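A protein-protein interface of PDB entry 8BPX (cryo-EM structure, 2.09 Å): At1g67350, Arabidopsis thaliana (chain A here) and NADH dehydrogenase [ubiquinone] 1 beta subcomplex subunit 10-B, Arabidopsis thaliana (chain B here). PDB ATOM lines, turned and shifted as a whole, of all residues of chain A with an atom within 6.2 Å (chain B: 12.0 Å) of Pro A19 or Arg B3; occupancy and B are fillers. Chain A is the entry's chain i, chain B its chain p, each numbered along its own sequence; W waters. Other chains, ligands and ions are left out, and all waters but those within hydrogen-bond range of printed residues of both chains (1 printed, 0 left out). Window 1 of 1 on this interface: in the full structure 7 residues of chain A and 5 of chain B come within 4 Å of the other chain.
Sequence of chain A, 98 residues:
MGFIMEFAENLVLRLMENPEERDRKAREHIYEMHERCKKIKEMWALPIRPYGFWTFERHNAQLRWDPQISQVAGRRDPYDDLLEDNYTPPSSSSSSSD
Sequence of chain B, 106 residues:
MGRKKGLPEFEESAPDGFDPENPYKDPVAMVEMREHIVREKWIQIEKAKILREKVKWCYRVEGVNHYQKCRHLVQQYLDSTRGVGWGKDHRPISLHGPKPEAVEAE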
ATOM      1  N   LEU A  13      22.571  -7.473 -11.454  1.00  0.00           N
ATOM      2  CA  LEU A  13      22.088  -8.877 -11.516  1.00  0.00           C
ATOM      3  C   LEU A  13      23.266  -9.854 -11.665  1.00  0.00           C
ATOM      4  O   LEU A  13      23.200 -10.940 -11.081  1.00  0.00           O
ATOM      5  CB  LEU A  13      21.077  -9.022 -12.659  1.00  0.00           C
ATOM      6  CG  LEU A  13      19.723  -8.350 -12.458  1.00  0.00           C
ATOM      7  CD1 LEU A  13      18.960  -8.296 -13.770  1.00  0.00           C
ATOM      8  CD2 LEU A  13      18.906  -9.062 -11.394  1.00  0.00           C
ATOM      9  N   ARG A  14      24.299  -9.470 -12.413  1.00  0.00           N
ATOM     10  CA  ARG A  14      25.520 -10.288 -12.624  1.00  0.00           C
ATOM     11  C   ARG A  14      26.317 -10.426 -11.314  1.00  0.00           C
ATOM     12  O   ARG A  14      26.985 -11.436 -11.153  1.00  0.00           O
ATOM     13  CB  ARG A  14      26.386  -9.678 -13.736  1.00  0.00           C
ATOM     14  CG  ARG A  14      26.250 -10.359 -15.087  1.00  0.00           C
ATOM     15  CD  ARG A  14      26.127  -9.351 -16.215  1.00  0.00           C
ATOM     16  NE  ARG A  14      27.143  -8.309 -16.146  1.00  0.00           N
ATOM     17  CZ  ARG A  14      27.036  -7.110 -16.705  1.00  0.00           C
ATOM     18  NH1 ARG A  14      25.950  -6.787 -17.384  1.00  0.00           N
ATOM     19  NH2 ARG A  14      28.018  -6.235 -16.586  1.00  0.00           N
ATOM     20  N   LEU A  15      26.210  -9.445 -10.417  1.00  0.00           N
ATOM     21  CA  LEU A  15      26.955  -9.444  -9.131  1.00  0.00           C
ATOM     22  C   LEU A  15      26.346 -10.440  -8.143  1.00  0.00           C
ATOM     23  O   LEU A  15      27.051 -10.867  -7.236  1.00  0.00           O
ATOM     24  CB  LEU A  15      26.943  -8.035  -8.554  1.00  0.00           C
ATOM     25  CG  LEU A  15      27.770  -7.005  -9.320  1.00  0.00           C
ATOM     26  CD1 LEU A  15      27.519  -5.606  -8.785  1.00  0.00           C
ATOM     27  CD2 LEU A  15      29.247  -7.343  -9.266  1.00  0.00           C
ATOM     28  N   MET A  16      25.074 -10.750  -8.320  1.00  0.00           N
ATOM     29  CA  MET A  16      24.227 -11.304  -7.237  1.00  0.00           C
ATOM     30  C   MET A  16      24.392 -12.823  -7.257  1.00  0.00           C
ATOM     31  O   MET A  16      24.836 -13.346  -8.276  1.00  0.00           O
ATOM     32  CB  MET A  16      22.765 -10.891  -7.426  1.00  0.00           C
ATOM     33  CG  MET A  16      22.480  -9.468  -7.013  1.00  0.00           C
ATOM     34  SD  MET A  16      20.746  -9.020  -7.228  1.00  0.00           S
ATOM     35  CE  MET A  16      20.451  -8.032  -5.766  1.00  0.00           C
ATOM     36  N   GLU A  17      24.155 -13.480  -6.129  1.00  0.00           N
ATOM     37  CA  GLU A  17      24.135 -14.964  -6.120  1.00  0.00           C
ATOM     38  C   GLU A  17      22.963 -15.442  -6.977  1.00  0.00           C
ATOM     39  O   GLU A  17      21.900 -14.791  -6.944  1.00  0.00           O
ATOM     40  CB  GLU A  17      23.996 -15.489  -4.698  1.00  0.00           C
ATOM     41  CG  GLU A  17      25.177 -15.174  -3.808  1.00  0.00           C
ATOM     42  CD  GLU A  17      25.064 -15.808  -2.434  1.00  0.00           C
ATOM     43  OE1 GLU A  17      25.578 -16.922  -2.266  1.00  0.00           O
ATOM     44  OE2 GLU A  17      24.443 -15.195  -1.549  1.00  0.00           O
ATOM     45  N   ASN A  18      23.183 -16.526  -7.716  1.00  0.00           N
ATOM     46  CA  ASN A  18      22.109 -17.440  -8.183  1.00  0.00           C
ATOM     47  C   ASN A  18      21.287 -17.982  -6.999  1.00  0.00           C
ATOM     48  O   ASN A  18      21.798 -18.840  -6.268  1.00  0.00           O
ATOM     49  CB  ASN A  18      22.684 -18.560  -9.054  1.00  0.00           C
ATOM     50  CG  ASN A  18      21.617 -19.324  -9.806  1.00  0.00           C
ATOM     51  OD1 ASN A  18      20.698 -19.871  -9.209  1.00  0.00           O
ATOM     52  ND2 ASN A  18      21.735 -19.368 -11.121  1.00  0.00           N
ATOM     53  N   PRO A  19      20.025 -17.538  -6.817  1.00  0.00           N
ATOM     54  CA  PRO A  19      19.210 -17.911  -5.639  1.00  0.00           C
ATOM     55  C   PRO A  19      18.931 -19.407  -5.506  1.00  0.00           C
ATOM     56  O   PRO A  19      18.903 -19.893  -4.411  1.00  0.00           O
ATOM     57  CB  PRO A  19      17.899 -17.131  -5.866  1.00  0.00           C
ATOM     58  CG  PRO A  19      17.867 -16.837  -7.343  1.00  0.00           C
ATOM     59  CD  PRO A  19      19.312 -16.651  -7.737  1.00  0.00           C
ATOM     60  N   GLU A  20      18.766 -20.079  -6.627  1.00  0.00           N
ATOM     61  CA  GLU A  20      18.549 -21.522  -6.665  1.00  0.00           C
ATOM     62  C   GLU A  20      19.748 -22.278  -6.102  1.00  0.00           C
ATOM     63  O   GLU A  20      19.601 -23.120  -5.209  1.00  0.00           O
ATOM     64  CB  GLU A  20      18.258 -21.969  -8.099  1.00  0.00           C
ATOM     65  CG  GLU A  20      16.802 -21.840  -8.522  1.00  0.00           C
ATOM     66  CD  GLU A  20      15.828 -22.238  -7.431  1.00  0.00           C
ATOM     67  OE1 GLU A  20      15.477 -23.433  -7.355  1.00  0.00           O
ATOM     68  OE2 GLU A  20      15.394 -21.354  -6.661  1.00  0.00           O
ATOM     69  N   GLU A  21      20.947 -21.982  -6.609  1.00  0.00           N
ATOM     70  CA  GLU A  21      22.141 -22.670  -6.127  1.00  0.00           C
ATOM     71  C   GLU A  21      22.439 -22.321  -4.673  1.00  0.00           C
ATOM     72  O   GLU A  21      22.881 -23.179  -3.903  1.00  0.00           O
ATOM     73  CB  GLU A  21      23.338 -22.337  -7.016  1.00  0.00           C
ATOM     74  CG  GLU A  21      23.245 -22.908  -8.423  1.00  0.00           C
ATOM     75  CD  GLU A  21      24.222 -22.257  -9.383  1.00  0.00           C
ATOM     76  OE1 GLU A  21      25.214 -21.663  -8.911  1.00  0.00           O
ATOM     77  OE2 GLU A  21      23.999 -22.341 -10.609  1.00  0.00           O
ATOM     78  N   ARG A  22      22.213 -21.060  -4.296  1.00  0.00           N
ATOM     79  CA  ARG A  22      22.479 -20.632  -2.897  1.00  0.00           C
ATOM     80  C   ARG A  22      21.563 -21.436  -1.953  1.00  0.00           C
ATOM     81  O   ARG A  22      22.093 -22.028  -1.001  1.00  0.00           O
ATOM     82  CB  ARG A  22      22.378 -19.115  -2.724  1.00  0.00           C
ATOM     83  CG  ARG A  22      22.553 -18.659  -1.284  1.00  0.00           C
ATOM     84  CD  ARG A  22      21.321 -17.977  -0.742  1.00  0.00           C
ATOM     85  NE  ARG A  22      21.058 -16.801  -1.548  1.00  0.00           N
ATOM     86  CZ  ARG A  22      19.888 -16.497  -2.085  1.00  0.00           C
ATOM     87  NH1 ARG A  22      18.841 -17.279  -1.890  1.00  0.00           N
ATOM     88  NH2 ARG A  22      19.772 -15.407  -2.814  1.00  0.00           N
ATOM     89  N   ASP A  23      20.260 -21.516  -2.249  1.00  0.00           N
ATOM     90  CA  ASP A  23      19.347 -22.275  -1.400  1.00  0.00           C
ATOM     91  C   ASP A  23      19.657 -23.765  -1.435  1.00  0.00           C
ATOM     92  O   ASP A  23      19.511 -24.454  -0.418  1.00  0.00           O
ATOM     93  CB  ASP A  23      17.903 -22.014  -1.821  1.00  0.00           C
ATOM     94  CG  ASP A  23      17.439 -20.616  -1.466  1.00  0.00           C
ATOM     95  OD1 ASP A  23      18.091 -19.972  -0.620  1.00  0.00           O
ATOM     96  OD2 ASP A  23      16.422 -20.160  -2.032  1.00  0.00           O
ATOM     97  N   ARG A  24      20.249 -24.427  -2.480  1.00  0.00           N
ATOM     98  CA  ARG A  24      20.662 -25.896  -2.584  1.00  0.00           C
ATOM     99  C   ARG A  24      21.954 -26.379  -1.814  1.00  0.00           C
ATOM    100  O   ARG A  24      21.930 -27.461  -1.197  1.00  0.00           O
ATOM    101  CB  ARG A  24      20.964 -26.413  -3.995  1.00  0.00           C
ATOM    102  CG  ARG A  24      21.135 -27.922  -4.040  1.00  0.00           C
ATOM    103  CD  ARG A  24      21.638 -28.597  -5.295  1.00  0.00           C
ATOM    104  NE  ARG A  24      22.802 -28.006  -5.914  1.00  0.00           N
ATOM    105  CZ  ARG A  24      24.023 -28.029  -5.409  1.00  0.00           C
ATOM    106  NH1 ARG A  24      24.254 -28.607  -4.242  1.00  0.00           N
ATOM    107  NH2 ARG A  24      25.005 -27.447  -6.064  1.00  0.00           N
ATOM    108  N   GLY B   2      24.588 -15.393 -10.747  1.00  0.00           N
ATOM    109  CA  GLY B   2      23.742 -14.345 -11.337  1.00  0.00           C
ATOM    110  C   GLY B   2      22.281 -14.577 -11.039  1.00  0.00           C
ATOM    111  O   GLY B   2      21.848 -15.730 -11.041  1.00  0.00           O
ATOM    112  N   ARG B   3      21.559 -13.489 -10.787  1.00  0.00           N
ATOM    113  CA  ARG B   3      20.096 -13.536 -10.694  1.00  0.00           C
ATOM    114  C   ARG B   3      19.558 -13.228 -12.100  1.00  0.00           C
ATOM    115  O   ARG B   3      19.872 -12.163 -12.643  1.00  0.00           O
ATOM    116  CB  ARG B   3      19.610 -12.561  -9.616  1.00  0.00           C
ATOM    117  CG  ARG B   3      18.141 -12.711  -9.264  1.00  0.00           C
ATOM    118  CD  ARG B   3      17.806 -11.943  -8.006  1.00  0.00           C
ATOM    119  NE  ARG B   3      17.524 -12.822  -6.885  1.00  0.00           N
ATOM    120  CZ  ARG B   3      16.339 -13.359  -6.635  1.00  0.00           C
ATOM    121  NH1 ARG B   3      15.316 -13.112  -7.434  1.00  0.00           N
ATOM    122  NH2 ARG B   3      16.177 -14.137  -5.582  1.00  0.00           N
ATOM    123  N   LYS B   4      18.695 -14.086 -12.613  1.00  0.00           N
ATOM    124  CA  LYS B   4      17.835 -13.716 -13.723  1.00  0.00           C
ATOM    125  C   LYS B   4      16.932 -12.548 -13.345  1.00  0.00           C
ATOM    126  O   LYS B   4      16.558 -12.366 -12.184  1.00  0.00           O
ATOM    127  CB  LYS B   4      16.990 -14.911 -14.155  1.00  0.00           C
ATOM    128  CG  LYS B   4      17.795 -16.041 -14.767  1.00  0.00           C
ATOM    129  CD  LYS B   4      16.907 -17.210 -15.154  1.00  0.00           C
ATOM    130  CE  LYS B   4      17.712 -18.333 -15.790  1.00  0.00           C
ATOM    131  NZ  LYS B   4      16.848 -19.493 -16.151  1.00  0.00           N
ATOM    132  N   LYS B   5      16.588 -11.747 -14.345  1.00  0.00           N
ATOM    133  CA  LYS B   5      15.660 -10.650 -14.133  1.00  0.00           C
ATOM    134  C   LYS B   5      14.285 -11.194 -13.770  1.00  0.00           C
ATOM    135  O   LYS B   5      13.848 -12.218 -14.298  1.00  0.00           O
ATOM    136  CB  LYS B   5      15.579  -9.783 -15.389  1.00  0.00           C
ATOM    137  CG  LYS B   5      14.596  -8.633 -15.299  1.00  0.00           C
ATOM    138  CD  LYS B   5      14.455  -7.922 -16.635  1.00  0.00           C
ATOM    139  CE  LYS B   5      14.327  -6.423 -16.447  1.00  0.00           C
ATOM    140  NZ  LYS B   5      15.428  -5.874 -15.607  1.00  0.00           N
ATOM    141  N   GLY B   6      13.612 -10.517 -12.847  1.00  0.00           N
ATOM    142  CA  GLY B   6      12.248 -10.851 -12.496  1.00  0.00           C
ATOM    143  C   GLY B   6      12.043 -10.921 -10.997  1.00  0.00           C
ATOM    144  O   GLY B   6      12.981 -10.905 -10.203  1.00  0.00           O
ATOM    145  N   LEU B   7      10.768 -11.007 -10.626  1.00  0.00           N
ATOM    146  CA  LEU B   7      10.404 -11.138  -9.225  1.00  0.00           C
ATOM    147  C   LEU B   7      10.865 -12.486  -8.671  1.00  0.00           C
ATOM    148  O   LEU B   7      10.993 -13.459  -9.415  1.00  0.00           O
ATOM    149  CB  LEU B   7       8.895 -11.002  -9.041  1.00  0.00           C
ATOM    150  CG  LEU B   7       8.305  -9.595  -9.004  1.00  0.00           C
ATOM    151  CD1 LEU B   7       8.158  -8.996 -10.403  1.00  0.00           C
ATOM    152  CD2 LEU B   7       6.980  -9.604  -8.257  1.00  0.00           C
ATOM    153  N   PRO B   8      11.120 -12.566  -7.367  1.00  0.00           N
ATOM    154  CA  PRO B   8      11.529 -13.847  -6.777  1.00  0.00           C
ATOM    155  C   PRO B   8      10.451 -14.904  -6.947  1.00  0.00           C
ATOM    156  O   PRO B   8       9.254 -14.616  -6.908  1.00  0.00           O
ATOM    157  CB  PRO B   8      11.754 -13.517  -5.295  1.00  0.00           C
ATOM    158  CG  PRO B   8      11.357 -12.128  -5.095  1.00  0.00           C
ATOM    159  CD  PRO B   8      11.056 -11.469  -6.389  1.00  0.00           C
ATOM    160  N   GLU B   9      10.886 -16.143  -7.130  1.00  0.00           N
ATOM    161  CA  GLU B   9       9.986 -17.271  -7.322  1.00  0.00           C
ATOM    162  C   GLU B   9      10.116 -18.231  -6.148  1.00  0.00           C
ATOM    163  O   GLU B   9      11.228 -18.580  -5.742  1.00  0.00           O
ATOM    164  CB  GLU B   9      10.282 -18.003  -8.630  1.00  0.00           C
ATOM    165  CG  GLU B   9      10.676 -17.102  -9.784  1.00  0.00           C
ATOM    166  CD  GLU B   9      12.162 -16.794  -9.790  1.00  0.00           C
ATOM    167  OE1 GLU B   9      12.961 -17.741  -9.629  1.00  0.00           O
ATOM    168  OE2 GLU B   9      12.533 -15.615  -9.951  1.00  0.00           O
ATOM    169  N   PHE B  10       8.990 -18.656  -5.643  1.00  0.00           N
ATOM    170  CA  PHE B  10       8.999 -19.659  -4.584  1.00  0.00           C
ATOM    171  C   PHE B  10       7.968 -20.753  -4.861  1.00  0.00           C
ATOM    172  O   PHE B  10       7.075 -20.534  -5.629  1.00  0.00           O
ATOM    173  CB  PHE B  10       8.762 -18.999  -3.230  1.00  0.00           C
ATOM    174  CG  PHE B  10       9.676 -17.882  -2.804  1.00  0.00           C
ATOM    175  CD1 PHE B  10      10.901 -18.151  -2.217  1.00  0.00           C
ATOM    176  CD2 PHE B  10       9.276 -16.559  -2.932  1.00  0.00           C
ATOM    177  CE1 PHE B  10      11.722 -17.119  -1.800  1.00  0.00           C
ATOM    178  CE2 PHE B  10      10.104 -15.531  -2.524  1.00  0.00           C
ATOM    179  CZ  PHE B  10      11.328 -15.810  -1.958  1.00  0.00           C
ATOM    180  N   GLU B  11       8.073 -21.893  -4.182  1.00  0.00           N
ATOM    181  CA  GLU B  11       7.041 -22.971  -4.289  1.00  0.00           C
ATOM    182  C   GLU B  11       5.719 -22.532  -3.646  1.00  0.00           C
ATOM    183  O   GLU B  11       5.725 -22.170  -2.453  1.00  0.00           O
ATOM    184  CB  GLU B  11       7.538 -24.226  -3.618  1.00  0.00           C
ATOM    185  CG  GLU B  11       6.511 -25.337  -3.505  1.00  0.00           C
ATOM    186  CD  GLU B  11       5.847 -25.760  -4.802  1.00  0.00           C
ATOM    187  OE1 GLU B  11       6.567 -26.215  -5.709  1.00  0.00           O
ATOM    188  OE2 GLU B  11       4.615 -25.616  -4.905  1.00  0.00           O
ATOM    189  N   GLU B  32      12.321 -25.062   5.695  1.00  0.00           N
ATOM    190  CA  GLU B  32      11.463 -24.706   4.570  1.00  0.00           C
ATOM    191  C   GLU B  32      10.060 -24.342   5.036  1.00  0.00           C
ATOM    192  O   GLU B  32       9.444 -23.414   4.505  1.00  0.00           O
ATOM    193  CB  GLU B  32      11.424 -25.848   3.552  1.00  0.00           C
ATOM    194  CG  GLU B  32      12.723 -26.140   2.753  1.00  0.00           C
ATOM    195  CD  GLU B  32      13.528 -24.921   2.257  1.00  0.00           C
ATOM    196  OE1 GLU B  32      13.242 -23.754   2.593  1.00  0.00           O
ATOM    197  OE2 GLU B  32      14.498 -25.151   1.506  1.00  0.00           O
ATOM    198  N   GLU B  35      10.085 -20.801   6.470  1.00  0.00           N
ATOM    199  CA  GLU B  35      10.093 -19.789   5.414  1.00  0.00           C
ATOM    200  C   GLU B  35       8.741 -19.698   4.710  1.00  0.00           C
ATOM    201  O   GLU B  35       8.267 -18.598   4.393  1.00  0.00           O
ATOM    202  CB  GLU B  35      11.208 -20.075   4.409  1.00  0.00           C
ATOM    203  CG  GLU B  35      12.523 -20.462   5.052  1.00  0.00           C
ATOM    204  CD  GLU B  35      13.632 -19.465   4.801  1.00  0.00           C
ATOM    205  OE1 GLU B  35      13.384 -18.245   4.903  1.00  0.00           O
ATOM    206  OE2 GLU B  35      14.761 -19.907   4.508  1.00  0.00           O
ATOM    207  N   ARG B  39       6.222 -16.457   4.443  1.00  0.00           N
ATOM    208  CA  ARG B  39       5.698 -15.942   3.181  1.00  0.00           C
ATOM    209  C   ARG B  39       4.174 -15.851   3.205  1.00  0.00           C
ATOM    210  O   ARG B  39       3.592 -14.864   2.730  1.00  0.00           O
ATOM    211  CB  ARG B  39       6.188 -16.818   2.029  1.00  0.00           C
ATOM    212  CG  ARG B  39       7.208 -16.132   1.138  1.00  0.00           C
ATOM    213  CD  ARG B  39       8.473 -16.931   0.928  1.00  0.00           C
ATOM    214  NE  ARG B  39       8.235 -18.334   0.614  1.00  0.00           N
ATOM    215  CZ  ARG B  39       9.164 -19.278   0.700  1.00  0.00           C
ATOM    216  NH1 ARG B  39      10.397 -18.999   1.083  1.00  0.00           N
ATOM    217  NH2 ARG B  39       8.846 -20.531   0.394  1.00  0.00           N
HETATM  218  O   HOH W   1      21.955 -11.917 -13.822  1.00  0.00           O
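The backbone NH (N) of Arg B3 sits at hydrogen-bond distance from the backbone carbonyl oxygen (O) of Leu A13.
N of Gly B2 lies within hydrogen-bond range of O of Met A16 (3.2 Å).
The backbone NH of Glu A20 sits at hydrogen-bond distance from the side-chain amide oxygen of Asn A18 (3.2 Å).
The backbone NH (N) of Glu A21 is in hydrogen-bond range of the side-chain amide oxygen (OD1) of Asn A18.
Among the printed residues, merely in contact across the chains: Asn A18 with Gly B2, Leu A13 with Gly B2 and Pro A19 with Arg B3.
Pro A19 touches one residue of chain B.
Of chain A, only Leu A13 and Pro A19 come within 4 Å of Arg B3.
Leu A13 touches two residues of chain B.
No residue of chain B comes within 4 Å of Glu A17.
Of chain B, only Gly B2 comes within 4 Å of Asn A18.
No residue of chain B comes within 4 Å of Arg A22.
Of the printed residues of chain A, Gly B2 touches Leu A13 (3.5 Å), Met A16 (3.2 Å) and Asn A18 (3.3 Å).
Glu B32 touches none of the printed residues of chain A.
Glu B35 touches none of the printed residues of chain A.
The nearest printed residue of chain A that does not touch Gly B2 is Glu A17 (4.1 Å).
Hydrophobic or aromatic side chains of chain A that line the printed part of chain B: Leu A13 and Pro A19.
Among the printed residues, no Asp or Glu carboxylate lies within 4 Å of a Lys or Arg side-chain nitrogen of the other chain.
Water W1 bridges O of Arg B3 (2.4 Å) and O of Leu A13 (3.2 Å).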
